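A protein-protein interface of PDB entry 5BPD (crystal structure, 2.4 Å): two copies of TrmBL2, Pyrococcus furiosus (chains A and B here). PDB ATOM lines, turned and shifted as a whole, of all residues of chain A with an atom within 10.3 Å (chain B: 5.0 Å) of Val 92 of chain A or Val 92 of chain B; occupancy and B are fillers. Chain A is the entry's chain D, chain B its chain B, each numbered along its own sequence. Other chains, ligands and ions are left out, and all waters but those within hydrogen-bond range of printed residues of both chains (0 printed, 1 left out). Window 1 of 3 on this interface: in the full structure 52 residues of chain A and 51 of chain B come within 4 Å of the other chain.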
ATOM      1  N   GLU A  15      23.746 -31.838 -19.783  1.00  0.00           N
ATOM      2  CA  GLU A  15      24.900 -30.990 -19.505  1.00  0.00           C
ATOM      3  C   GLU A  15      25.876 -31.592 -18.499  1.00  0.00           C
ATOM      4  O   GLU A  15      26.556 -30.862 -17.778  1.00  0.00           O
ATOM      5  CB  GLU A  15      24.430 -29.623 -18.999  1.00  0.00           C
ATOM      6  CG  GLU A  15      23.832 -28.735 -20.076  1.00  0.00           C
ATOM      7  CD  GLU A  15      23.250 -27.453 -19.515  1.00  0.00           C
ATOM      8  OE1 GLU A  15      23.899 -26.839 -18.642  1.00  0.00           O
ATOM      9  OE2 GLU A  15      22.147 -27.056 -19.948  1.00  0.00           O
ATOM     10  N   PHE A  84      15.640 -30.728 -13.856  1.00  0.00           N
ATOM     11  CA  PHE A  84      16.549 -30.102 -14.811  1.00  0.00           C
ATOM     12  C   PHE A  84      15.787 -29.461 -15.964  1.00  0.00           C
ATOM     13  O   PHE A  84      16.088 -28.341 -16.371  1.00  0.00           O
ATOM     14  CB  PHE A  84      17.554 -31.118 -15.370  1.00  0.00           C
ATOM     15  CG  PHE A  84      18.520 -30.525 -16.361  1.00  0.00           C
ATOM     16  CD1 PHE A  84      18.151 -30.339 -17.687  1.00  0.00           C
ATOM     17  CD2 PHE A  84      19.797 -30.158 -15.970  1.00  0.00           C
ATOM     18  CE1 PHE A  84      19.029 -29.785 -18.598  1.00  0.00           C
ATOM     19  CE2 PHE A  84      20.686 -29.611 -16.881  1.00  0.00           C
ATOM     20  CZ  PHE A  84      20.301 -29.426 -18.198  1.00  0.00           C
ATOM     21  N   ILE A  85      14.810 -30.184 -16.497  1.00  0.00           N
ATOM     22  CA  ILE A  85      14.031 -29.697 -17.628  1.00  0.00           C
ATOM     23  C   ILE A  85      13.192 -28.500 -17.210  1.00  0.00           C
ATOM     24  O   ILE A  85      13.048 -27.538 -17.967  1.00  0.00           O
ATOM     25  CB  ILE A  85      13.152 -30.809 -18.212  1.00  0.00           C
ATOM     26  CG1 ILE A  85      14.034 -31.935 -18.757  1.00  0.00           C
ATOM     27  CG2 ILE A  85      12.235 -30.245 -19.296  1.00  0.00           C
ATOM     28  CD1 ILE A  85      13.265 -33.106 -19.317  1.00  0.00           C
ATOM     29  N   GLN A  86      12.640 -28.564 -16.000  1.00  0.00           N
ATOM     30  CA  GLN A  86      11.868 -27.454 -15.462  1.00  0.00           C
ATOM     31  C   GLN A  86      12.717 -26.190 -15.431  1.00  0.00           C
ATOM     32  O   GLN A  86      12.350 -25.172 -16.017  1.00  0.00           O
ATOM     33  CB  GLN A  86      11.355 -27.780 -14.061  1.00  0.00           C
ATOM     34  CG  GLN A  86      10.259 -28.829 -14.033  1.00  0.00           C
ATOM     35  CD  GLN A  86       9.774 -29.119 -12.629  1.00  0.00           C
ATOM     36  OE1 GLN A  86      10.504 -28.928 -11.656  1.00  0.00           O
ATOM     37  NE2 GLN A  86       8.535 -29.582 -12.516  1.00  0.00           N
ATOM     38  N   ASP A  87      13.863 -26.268 -14.764  1.00  0.00           N
ATOM     39  CA  ASP A  87      14.752 -25.120 -14.639  1.00  0.00           C
ATOM     40  C   ASP A  87      15.212 -24.627 -16.004  1.00  0.00           C
ATOM     41  O   ASP A  87      15.459 -23.434 -16.187  1.00  0.00           O
ATOM     42  CB  ASP A  87      15.961 -25.462 -13.766  1.00  0.00           C
ATOM     43  CG  ASP A  87      15.585 -25.670 -12.311  1.00  0.00           C
ATOM     44  OD1 ASP A  87      14.397 -25.939 -12.035  1.00  0.00           O
ATOM     45  OD2 ASP A  87      16.475 -25.555 -11.443  1.00  0.00           O
ATOM     46  N   TRP A  88      15.321 -25.545 -16.958  1.00  0.00           N
ATOM     47  CA  TRP A  88      15.740 -25.188 -18.307  1.00  0.00           C
ATOM     48  C   TRP A  88      14.609 -24.455 -19.018  1.00  0.00           C
ATOM     49  O   TRP A  88      14.829 -23.428 -19.662  1.00  0.00           O
ATOM     50  CB  TRP A  88      16.155 -26.435 -19.092  1.00  0.00           C
ATOM     51  CG  TRP A  88      16.625 -26.138 -20.482  1.00  0.00           C
ATOM     52  CD1 TRP A  88      17.898 -25.836 -20.869  1.00  0.00           C
ATOM     53  CD2 TRP A  88      15.826 -26.107 -21.670  1.00  0.00           C
ATOM     54  NE1 TRP A  88      17.942 -25.622 -22.226  1.00  0.00           N
ATOM     55  CE2 TRP A  88      16.684 -25.782 -22.740  1.00  0.00           C
ATOM     56  CE3 TRP A  88      14.469 -26.325 -21.932  1.00  0.00           C
ATOM     57  CZ2 TRP A  88      16.229 -25.669 -24.053  1.00  0.00           C
ATOM     58  CZ3 TRP A  88      14.018 -26.210 -23.235  1.00  0.00           C
ATOM     59  CH2 TRP A  88      14.895 -25.886 -24.279  1.00  0.00           C
ATOM     60  N   GLN A  89      13.394 -24.982 -18.885  1.00  0.00           N
ATOM     61  CA  GLN A  89      12.200 -24.301 -19.386  1.00  0.00           C
ATOM     62  C   GLN A  89      12.052 -22.924 -18.744  1.00  0.00           C
ATOM     63  O   GLN A  89      11.556 -21.983 -19.367  1.00  0.00           O
ATOM     64  CB  GLN A  89      10.945 -25.137 -19.122  1.00  0.00           C
ATOM     65  CG  GLN A  89      10.753 -26.283 -20.095  1.00  0.00           C
ATOM     66  CD  GLN A  89       9.494 -27.073 -19.819  1.00  0.00           C
ATOM     67  OE1 GLN A  89       8.688 -27.308 -20.716  1.00  0.00           O
ATOM     68  NE2 GLN A  89       9.323 -27.496 -18.573  1.00  0.00           N
ATOM     69  N   GLU A  90      12.472 -22.819 -17.489  1.00  0.00           N
ATOM     70  CA  GLU A  90      12.394 -21.562 -16.760  1.00  0.00           C
ATOM     71  C   GLU A  90      13.358 -20.543 -17.360  1.00  0.00           C
ATOM     72  O   GLU A  90      12.989 -19.394 -17.593  1.00  0.00           O
ATOM     73  CB  GLU A  90      12.697 -21.778 -15.276  1.00  0.00           C
ATOM     74  CG  GLU A  90      12.310 -20.613 -14.384  1.00  0.00           C
ATOM     75  CD  GLU A  90      10.806 -20.434 -14.284  1.00  0.00           C
ATOM     76  OE1 GLU A  90      10.069 -21.212 -14.929  1.00  0.00           O
ATOM     77  OE2 GLU A  90      10.358 -19.521 -13.559  1.00  0.00           O
ATOM     78  N   ARG A  91      14.595 -20.970 -17.609  1.00  0.00           N
ATOM     79  CA  ARG A  91      15.616 -20.076 -18.150  1.00  0.00           C
ATOM     80  C   ARG A  91      15.288 -19.656 -19.581  1.00  0.00           C
ATOM     81  O   ARG A  91      15.605 -18.543 -20.005  1.00  0.00           O
ATOM     82  CB  ARG A  91      16.994 -20.736 -18.096  1.00  0.00           C
ATOM     83  CG  ARG A  91      17.421 -21.158 -16.699  1.00  0.00           C
ATOM     84  CD  ARG A  91      18.893 -21.556 -16.653  1.00  0.00           C
ATOM     85  NE  ARG A  91      19.220 -22.628 -17.590  1.00  0.00           N
ATOM     86  CZ  ARG A  91      19.161 -23.923 -17.294  1.00  0.00           C
ATOM     87  NH1 ARG A  91      18.775 -24.308 -16.085  1.00  0.00           N
ATOM     88  NH2 ARG A  91      19.482 -24.832 -18.209  1.00  0.00           N
ATOM     89  N   VAL A  92      14.653 -20.556 -20.322  1.00  0.00           N
ATOM     90  CA  VAL A  92      14.219 -20.257 -21.681  1.00  0.00           C
ATOM     91  C   VAL A  92      13.135 -19.180 -21.668  1.00  0.00           C
ATOM     92  O   VAL A  92      13.157 -18.259 -22.483  1.00  0.00           O
ATOM     93  CB  VAL A  92      13.728 -21.528 -22.393  1.00  0.00           C
ATOM     94  CG1 VAL A  92      12.992 -21.167 -23.669  1.00  0.00           C
ATOM     95  CG2 VAL A  92      14.903 -22.439 -22.703  1.00  0.00           C
ATOM     96  N   LYS A  93      12.188 -19.302 -20.740  1.00  0.00           N
ATOM     97  CA  LYS A  93      11.135 -18.304 -20.572  1.00  0.00           C
ATOM     98  C   LYS A  93      11.729 -16.940 -20.253  1.00  0.00           C
ATOM     99  O   LYS A  93      11.278 -15.921 -20.768  1.00  0.00           O
ATOM    100  CB  LYS A  93      10.163 -18.726 -19.467  1.00  0.00           C
ATOM    101  CG  LYS A  93       9.135 -19.757 -19.903  1.00  0.00           C
ATOM    102  CD  LYS A  93       8.780 -20.709 -18.767  1.00  0.00           C
ATOM    103  CE  LYS A  93       8.308 -19.972 -17.527  1.00  0.00           C
ATOM    104  NZ  LYS A  93       7.991 -20.925 -16.424  1.00  0.00           N
ATOM    105  N   GLU A  94      12.752 -16.927 -19.405  1.00  0.00           N
ATOM    106  CA  GLU A  94      13.420 -15.686 -19.041  1.00  0.00           C
ATOM    107  C   GLU A  94      14.098 -15.064 -20.258  1.00  0.00           C
ATOM    108  O   GLU A  94      14.024 -13.854 -20.466  1.00  0.00           O
ATOM    109  CB  GLU A  94      14.439 -15.929 -17.925  1.00  0.00           C
ATOM    110  CG  GLU A  94      13.852 -16.605 -16.693  1.00  0.00           C
ATOM    111  CD  GLU A  94      14.833 -16.688 -15.537  1.00  0.00           C
ATOM    112  OE1 GLU A  94      15.446 -15.654 -15.201  1.00  0.00           O
ATOM    113  OE2 GLU A  94      14.990 -17.789 -14.967  1.00  0.00           O
ATOM    114  N   GLU A  95      14.749 -15.895 -21.069  1.00  0.00           N
ATOM    115  CA  GLU A  95      15.445 -15.395 -22.246  1.00  0.00           C
ATOM    116  C   GLU A  95      14.461 -14.907 -23.299  1.00  0.00           C
ATOM    117  O   GLU A  95      14.683 -13.876 -23.929  1.00  0.00           O
ATOM    118  CB  GLU A  95      16.358 -16.471 -22.840  1.00  0.00           C
ATOM    119  CG  GLU A  95      17.122 -16.012 -24.071  1.00  0.00           C
ATOM    120  CD  GLU A  95      18.004 -14.806 -23.793  1.00  0.00           C
ATOM    121  OE1 GLU A  95      18.345 -14.578 -22.613  1.00  0.00           O
ATOM    122  OE2 GLU A  95      18.357 -14.086 -24.751  1.00  0.00           O
ATOM    123  N   LEU A  96      13.374 -15.645 -23.491  1.00  0.00           N
ATOM    124  CA  LEU A  96      12.364 -15.242 -24.465  1.00  0.00           C
ATOM    125  C   LEU A  96      11.840 -13.845 -24.168  1.00  0.00           C
ATOM    126  O   LEU A  96      11.564 -13.065 -25.081  1.00  0.00           O
ATOM    127  CB  LEU A  96      11.199 -16.230 -24.489  1.00  0.00           C
ATOM    128  CG  LEU A  96      10.022 -15.775 -25.359  1.00  0.00           C
ATOM    129  CD1 LEU A  96      10.484 -15.487 -26.780  1.00  0.00           C
ATOM    130  CD2 LEU A  96       8.906 -16.808 -25.351  1.00  0.00           C
ATOM    131  N   GLU A  97      11.703 -13.532 -22.885  1.00  0.00           N
ATOM    132  CA  GLU A  97      11.216 -12.223 -22.474  1.00  0.00           C
ATOM    133  C   GLU A  97      12.291 -11.159 -22.675  1.00  0.00           C
ATOM    134  O   GLU A  97      11.996 -10.030 -23.063  1.00  0.00           O
ATOM    135  CB  GLU A  97      10.760 -12.253 -21.015  1.00  0.00           C
ATOM    136  CG  GLU A  97       9.712 -11.208 -20.691  1.00  0.00           C
ATOM    137  CD  GLU A  97       8.472 -11.346 -21.554  1.00  0.00           C
ATOM    138  OE1 GLU A  97       8.374 -12.342 -22.304  1.00  0.00           O
ATOM    139  OE2 GLU A  97       7.596 -10.459 -21.487  1.00  0.00           O
ATOM    140  N   ALA A  98      13.538 -11.523 -22.398  1.00  0.00           N
ATOM    141  CA  ALA A  98      14.663 -10.618 -22.606  1.00  0.00           C
ATOM    142  C   ALA A  98      14.842 -10.284 -24.087  1.00  0.00           C
ATOM    143  O   ALA A  98      15.215  -9.164 -24.435  1.00  0.00           O
ATOM    144  CB  ALA A  98      15.938 -11.218 -22.035  1.00  0.00           C
ATOM    145  N   LYS A  99      14.580 -11.260 -24.954  1.00  0.00           N
ATOM    146  CA  LYS A  99      14.655 -11.050 -26.399  1.00  0.00           C
ATOM    147  C   LYS A  99      13.602 -10.039 -26.850  1.00  0.00           C
ATOM    148  O   LYS A  99      13.900  -9.118 -27.609  1.00  0.00           O
ATOM    149  CB  LYS A  99      14.480 -12.374 -27.152  1.00  0.00           C
ATOM    150  CG  LYS A  99      15.744 -13.231 -27.233  1.00  0.00           C
ATOM    151  CD  LYS A  99      15.451 -14.602 -27.837  1.00  0.00           C
ATOM    152  CE  LYS A  99      16.722 -15.310 -28.303  1.00  0.00           C
ATOM    153  NZ  LYS A  99      17.773 -15.372 -27.249  1.00  0.00           N
ATOM    154  N   LYS A 100      12.370 -10.219 -26.381  1.00  0.00           N
ATOM    155  CA  LYS A 100      11.274  -9.310 -26.718  1.00  0.00           C
ATOM    156  C   LYS A 100      11.551  -7.902 -26.196  1.00  0.00           C
ATOM    157  O   LYS A 100      11.142  -6.913 -26.806  1.00  0.00           O
ATOM    158  CB  LYS A 100       9.947  -9.824 -26.156  1.00  0.00           C
ATOM    159  CG  LYS A 100       9.487 -11.148 -26.749  1.00  0.00           C
ATOM    160  CD  LYS A 100       8.070 -11.489 -26.304  1.00  0.00           C
ATOM    161  CE  LYS A 100       7.626 -12.837 -26.855  1.00  0.00           C
ATOM    162  NZ  LYS A 100       6.217 -13.153 -26.492  1.00  0.00           N
ATOM    163  N   TRP B  88      13.596 -18.859 -33.185  1.00  0.00           N
ATOM    164  CA  TRP B  88      14.240 -19.294 -31.953  1.00  0.00           C
ATOM    165  C   TRP B  88      13.281 -20.123 -31.102  1.00  0.00           C
ATOM    166  O   TRP B  88      13.675 -21.118 -30.493  1.00  0.00           O
ATOM    167  CB  TRP B  88      14.744 -18.079 -31.172  1.00  0.00           C
ATOM    168  CG  TRP B  88      15.320 -18.400 -29.828  1.00  0.00           C
ATOM    169  CD1 TRP B  88      16.613 -18.738 -29.549  1.00  0.00           C
ATOM    170  CD2 TRP B  88      14.629 -18.389 -28.572  1.00  0.00           C
ATOM    171  NE1 TRP B  88      16.767 -18.944 -28.202  1.00  0.00           N
ATOM    172  CE2 TRP B  88      15.566 -18.737 -27.579  1.00  0.00           C
ATOM    173  CE3 TRP B  88      13.312 -18.120 -28.193  1.00  0.00           C
ATOM    174  CZ2 TRP B  88      15.225 -18.826 -26.230  1.00  0.00           C
ATOM    175  CZ3 TRP B  88      12.976 -18.208 -26.856  1.00  0.00           C
ATOM    176  CH2 TRP B  88      13.929 -18.559 -25.890  1.00  0.00           C
ATOM    177  N   GLN B  89      12.017 -19.712 -31.074  1.00  0.00           N
ATOM    178  CA  GLN B  89      11.004 -20.402 -30.283  1.00  0.00           C
ATOM    179  C   GLN B  89      10.730 -21.813 -30.794  1.00  0.00           C
ATOM    180  O   GLN B  89      10.417 -22.709 -30.012  1.00  0.00           O
ATOM    181  CB  GLN B  89       9.706 -19.591 -30.254  1.00  0.00           C
ATOM    182  CG  GLN B  89       9.726 -18.457 -29.244  1.00  0.00           C
ATOM    183  CD  GLN B  89       8.396 -17.733 -29.144  1.00  0.00           C
ATOM    184  OE1 GLN B  89       8.039 -17.215 -28.088  1.00  0.00           O
ATOM    185  NE2 GLN B  89       7.665 -17.681 -30.251  1.00  0.00           N
ATOM    186  N   GLU B  90      10.842 -22.007 -32.105  1.00  0.00           N
ATOM    187  CA  GLU B  90      10.661 -23.332 -32.695  1.00  0.00           C
ATOM    188  C   GLU B  90      11.828 -24.252 -32.347  1.00  0.00           C
ATOM    189  O   GLU B  90      11.633 -25.431 -32.058  1.00  0.00           O
ATOM    190  CB  GLU B  90      10.502 -23.233 -34.212  1.00  0.00           C
ATOM    191  CG  GLU B  90       9.130 -22.765 -34.655  1.00  0.00           C
ATOM    192  CD  GLU B  90       8.958 -22.814 -36.160  1.00  0.00           C
ATOM    193  OE1 GLU B  90       8.924 -21.737 -36.791  1.00  0.00           O
ATOM    194  OE2 GLU B  90       8.853 -23.930 -36.710  1.00  0.00           O
ATOM    195  N   ARG B  91      13.040 -23.707 -32.381  1.00  0.00           N
ATOM    196  CA  ARG B  91      14.234 -24.466 -32.016  1.00  0.00           C
ATOM    197  C   ARG B  91      14.184 -24.900 -30.553  1.00  0.00           C
ATOM    198  O   ARG B  91      14.575 -26.018 -30.214  1.00  0.00           O
ATOM    199  CB  ARG B  91      15.497 -23.640 -32.274  1.00  0.00           C
ATOM    200  CG  ARG B  91      15.941 -23.609 -33.729  1.00  0.00           C
ATOM    201  CD  ARG B  91      17.184 -22.749 -33.901  1.00  0.00           C
ATOM    202  NE  ARG B  91      16.858 -21.326 -33.947  1.00  0.00           N
ATOM    203  CZ  ARG B  91      17.708 -20.352 -33.641  1.00  0.00           C
ATOM    204  NH1 ARG B  91      18.939 -20.645 -33.241  1.00  0.00           N
ATOM    205  NH2 ARG B  91      17.322 -19.085 -33.719  1.00  0.00           N
ATOM    206  N   VAL B  92      13.700 -24.010 -29.690  1.00  0.00           N
ATOM    207  CA  VAL B  92      13.598 -24.305 -28.263  1.00  0.00           C
ATOM    208  C   VAL B  92      12.569 -25.401 -28.015  1.00  0.00           C
ATOM    209  O   VAL B  92      12.753 -26.251 -27.144  1.00  0.00           O
ATOM    210  CB  VAL B  92      13.258 -23.039 -27.455  1.00  0.00           C
ATOM    211  CG1 VAL B  92      12.905 -23.406 -26.030  1.00  0.00           C
ATOM    212  CG2 VAL B  92      14.431 -22.075 -27.471  1.00  0.00           C
ATOM    213  N   LYS B  93      11.484 -25.377 -28.782  1.00  0.00           N
ATOM    214  CA  LYS B  93      10.456 -26.407 -28.681  1.00  0.00           C
ATOM    215  C   LYS B  93      11.024 -27.774 -29.042  1.00  0.00           C
ATOM    216  O   LYS B  93      10.741 -28.769 -28.378  1.00  0.00           O
ATOM    217  CB  LYS B  93       9.266 -26.082 -29.585  1.00  0.00           C
ATOM    218  CG  LYS B  93       8.393 -27.288 -29.904  1.00  0.00           C
ATOM    219  CD  LYS B  93       7.238 -26.921 -30.822  1.00  0.00           C
ATOM    220  CE  LYS B  93       6.587 -28.162 -31.419  1.00  0.00           C
ATOM    221  NZ  LYS B  93       6.110 -29.112 -30.376  1.00  0.00           N
ATOM    222  N   GLU B  94      11.823 -27.820 -30.103  1.00  0.00           N
ATOM    223  CA  GLU B  94      12.418 -29.076 -30.546  1.00  0.00           C
ATOM    224  C   GLU B  94      13.397 -29.610 -29.511  1.00  0.00           C
ATOM    225  O   GLU B  94      13.424 -30.808 -29.235  1.00  0.00           O
ATOM    226  CB  GLU B  94      13.120 -28.900 -31.894  1.00  0.00           C
ATOM    227  CG  GLU B  94      12.172 -28.838 -33.081  1.00  0.00           C
ATOM    228  CD  GLU B  94      12.883 -28.499 -34.376  1.00  0.00           C
ATOM    229  OE1 GLU B  94      14.133 -28.523 -34.391  1.00  0.00           O
ATOM    230  OE2 GLU B  94      12.194 -28.208 -35.378  1.00  0.00           O
ATOM    231  N   GLU B  95      14.201 -28.720 -28.938  1.00  0.00           N
ATOM    232  CA  GLU B  95      15.168 -29.122 -27.926  1.00  0.00           C
ATOM    233  C   GLU B  95      14.446 -29.642 -26.682  1.00  0.00           C
ATOM    234  O   GLU B  95      14.914 -30.578 -26.028  1.00  0.00           O
ATOM    235  CB  GLU B  95      16.095 -27.958 -27.571  1.00  0.00           C
ATOM    236  CG  GLU B  95      17.252 -28.343 -26.662  1.00  0.00           C
ATOM    237  CD  GLU B  95      18.258 -27.222 -26.488  1.00  0.00           C
ATOM    238  OE1 GLU B  95      18.109 -26.176 -27.156  1.00  0.00           O
ATOM    239  OE2 GLU B  95      19.200 -27.385 -25.685  1.00  0.00           O
ATOM    240  N   LEU B  96      13.307 -29.031 -26.362  1.00  0.00           N
ATOM    241  CA  LEU B  96      12.488 -29.471 -25.234  1.00  0.00           C
ATOM    242  C   LEU B  96      11.927 -30.869 -25.477  1.00  0.00           C
ATOM    243  O   LEU B  96      11.911 -31.707 -24.575  1.00  0.00           O
ATOM    244  CB  LEU B  96      11.343 -28.486 -24.971  1.00  0.00           C
ATOM    245  CG  LEU B  96      10.364 -28.892 -23.863  1.00  0.00           C
ATOM    246  CD1 LEU B  96      11.065 -28.977 -22.517  1.00  0.00           C
ATOM    247  CD2 LEU B  96       9.187 -27.932 -23.789  1.00  0.00           C
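The side-chain carboxylate (OE2) of Glu 95 of chain A lies within salt-bridge range of the side-chain amino group (NZ) of Lys 99 of chain A (2.9 Å).
Among the printed residues, merely in contact across the chains: Ile 85 of chain A with Leu 96 of chain B (3.7 Å), Trp 88 of chain A with Val 92 of chain B (3.6 Å), Trp 88 of chain A with Glu 95 of chain B (3.5 Å), Trp 88 of chain A with Leu 96 of chain B (3.9 Å), Gln 89 of chain A with Leu 96 of chain B (3.2 Å), Val 92 of chain A with Trp 88 of chain B (3.5 Å), Val 92 of chain A with Val 92 of chain B (3.3 Å), Leu 96 of chain A with Trp 88 of chain B (3.6 Å), Leu 96 of chain A with Gln 89 of chain B (2.9 Å) and Lys 99 of chain A with Trp 88 of chain B (3.6 Å).
Of the printed residues of chain B, Trp 88 of chain A touches Val 92 (3.6 Å), Glu 95 (3.5 Å) and Leu 96 (3.9 Å). Printed residues of chain B within 4 Å of Gln 89 of chain A: Leu 96 (3.2 Å). Val 92 of chain A touches two residues of chain B. Glu 95 of chain A touches none of the printed residues of chain B. Of the printed residues of chain A, Gln 89 of chain B touches Leu 96. Val 92 of chain B touches two residues of chain A. Of chain A, only Ile 85, Trp 88 and Gln 89 come within 4 Å of Leu 96 of chain B. The nearest printed residue of chain A that does not touch Val 92 of chain B is Lys 93 of chain A (6.7 Å). The nearest printed residue of chain B that does not touch Trp 88 of chain A is Lys 93 of chain B (5.7 Å).
Printed residues of chain B that touch a printed residue of chain A: Trp 88, Gln 89, Val 92, Glu 95 and Leu 96. Of the 18 printed residues of chain A, 6 touch a printed residue of chain B. Hydrophobic or aromatic side chains of chain A that line the printed part of chain B: Ile 85, Trp 88, Val 92 and Leu 96. Among the printed residues, 10 pairs touch across the chains.
Trp 88 of chain A touches Val 92 of chain B, and with the chains exchanged Val 92 of chain A touches Trp 88 of chain B. Trp 88 of chain A touches Leu 96 of chain B, and with the chains exchanged Leu 96 of chain A touches Trp 88 of chain B. Gln 89 of chain A touches Leu 96 of chain B, and with the chains exchanged Leu 96 of chain A touches Gln 89 of chain B. Val 92 of chain A touches its own counterpart, Val 92 of chain B. Of the 10 pairs that touch across the chains among the printed residues, 7 have their exchanged pair printed and touching as well.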
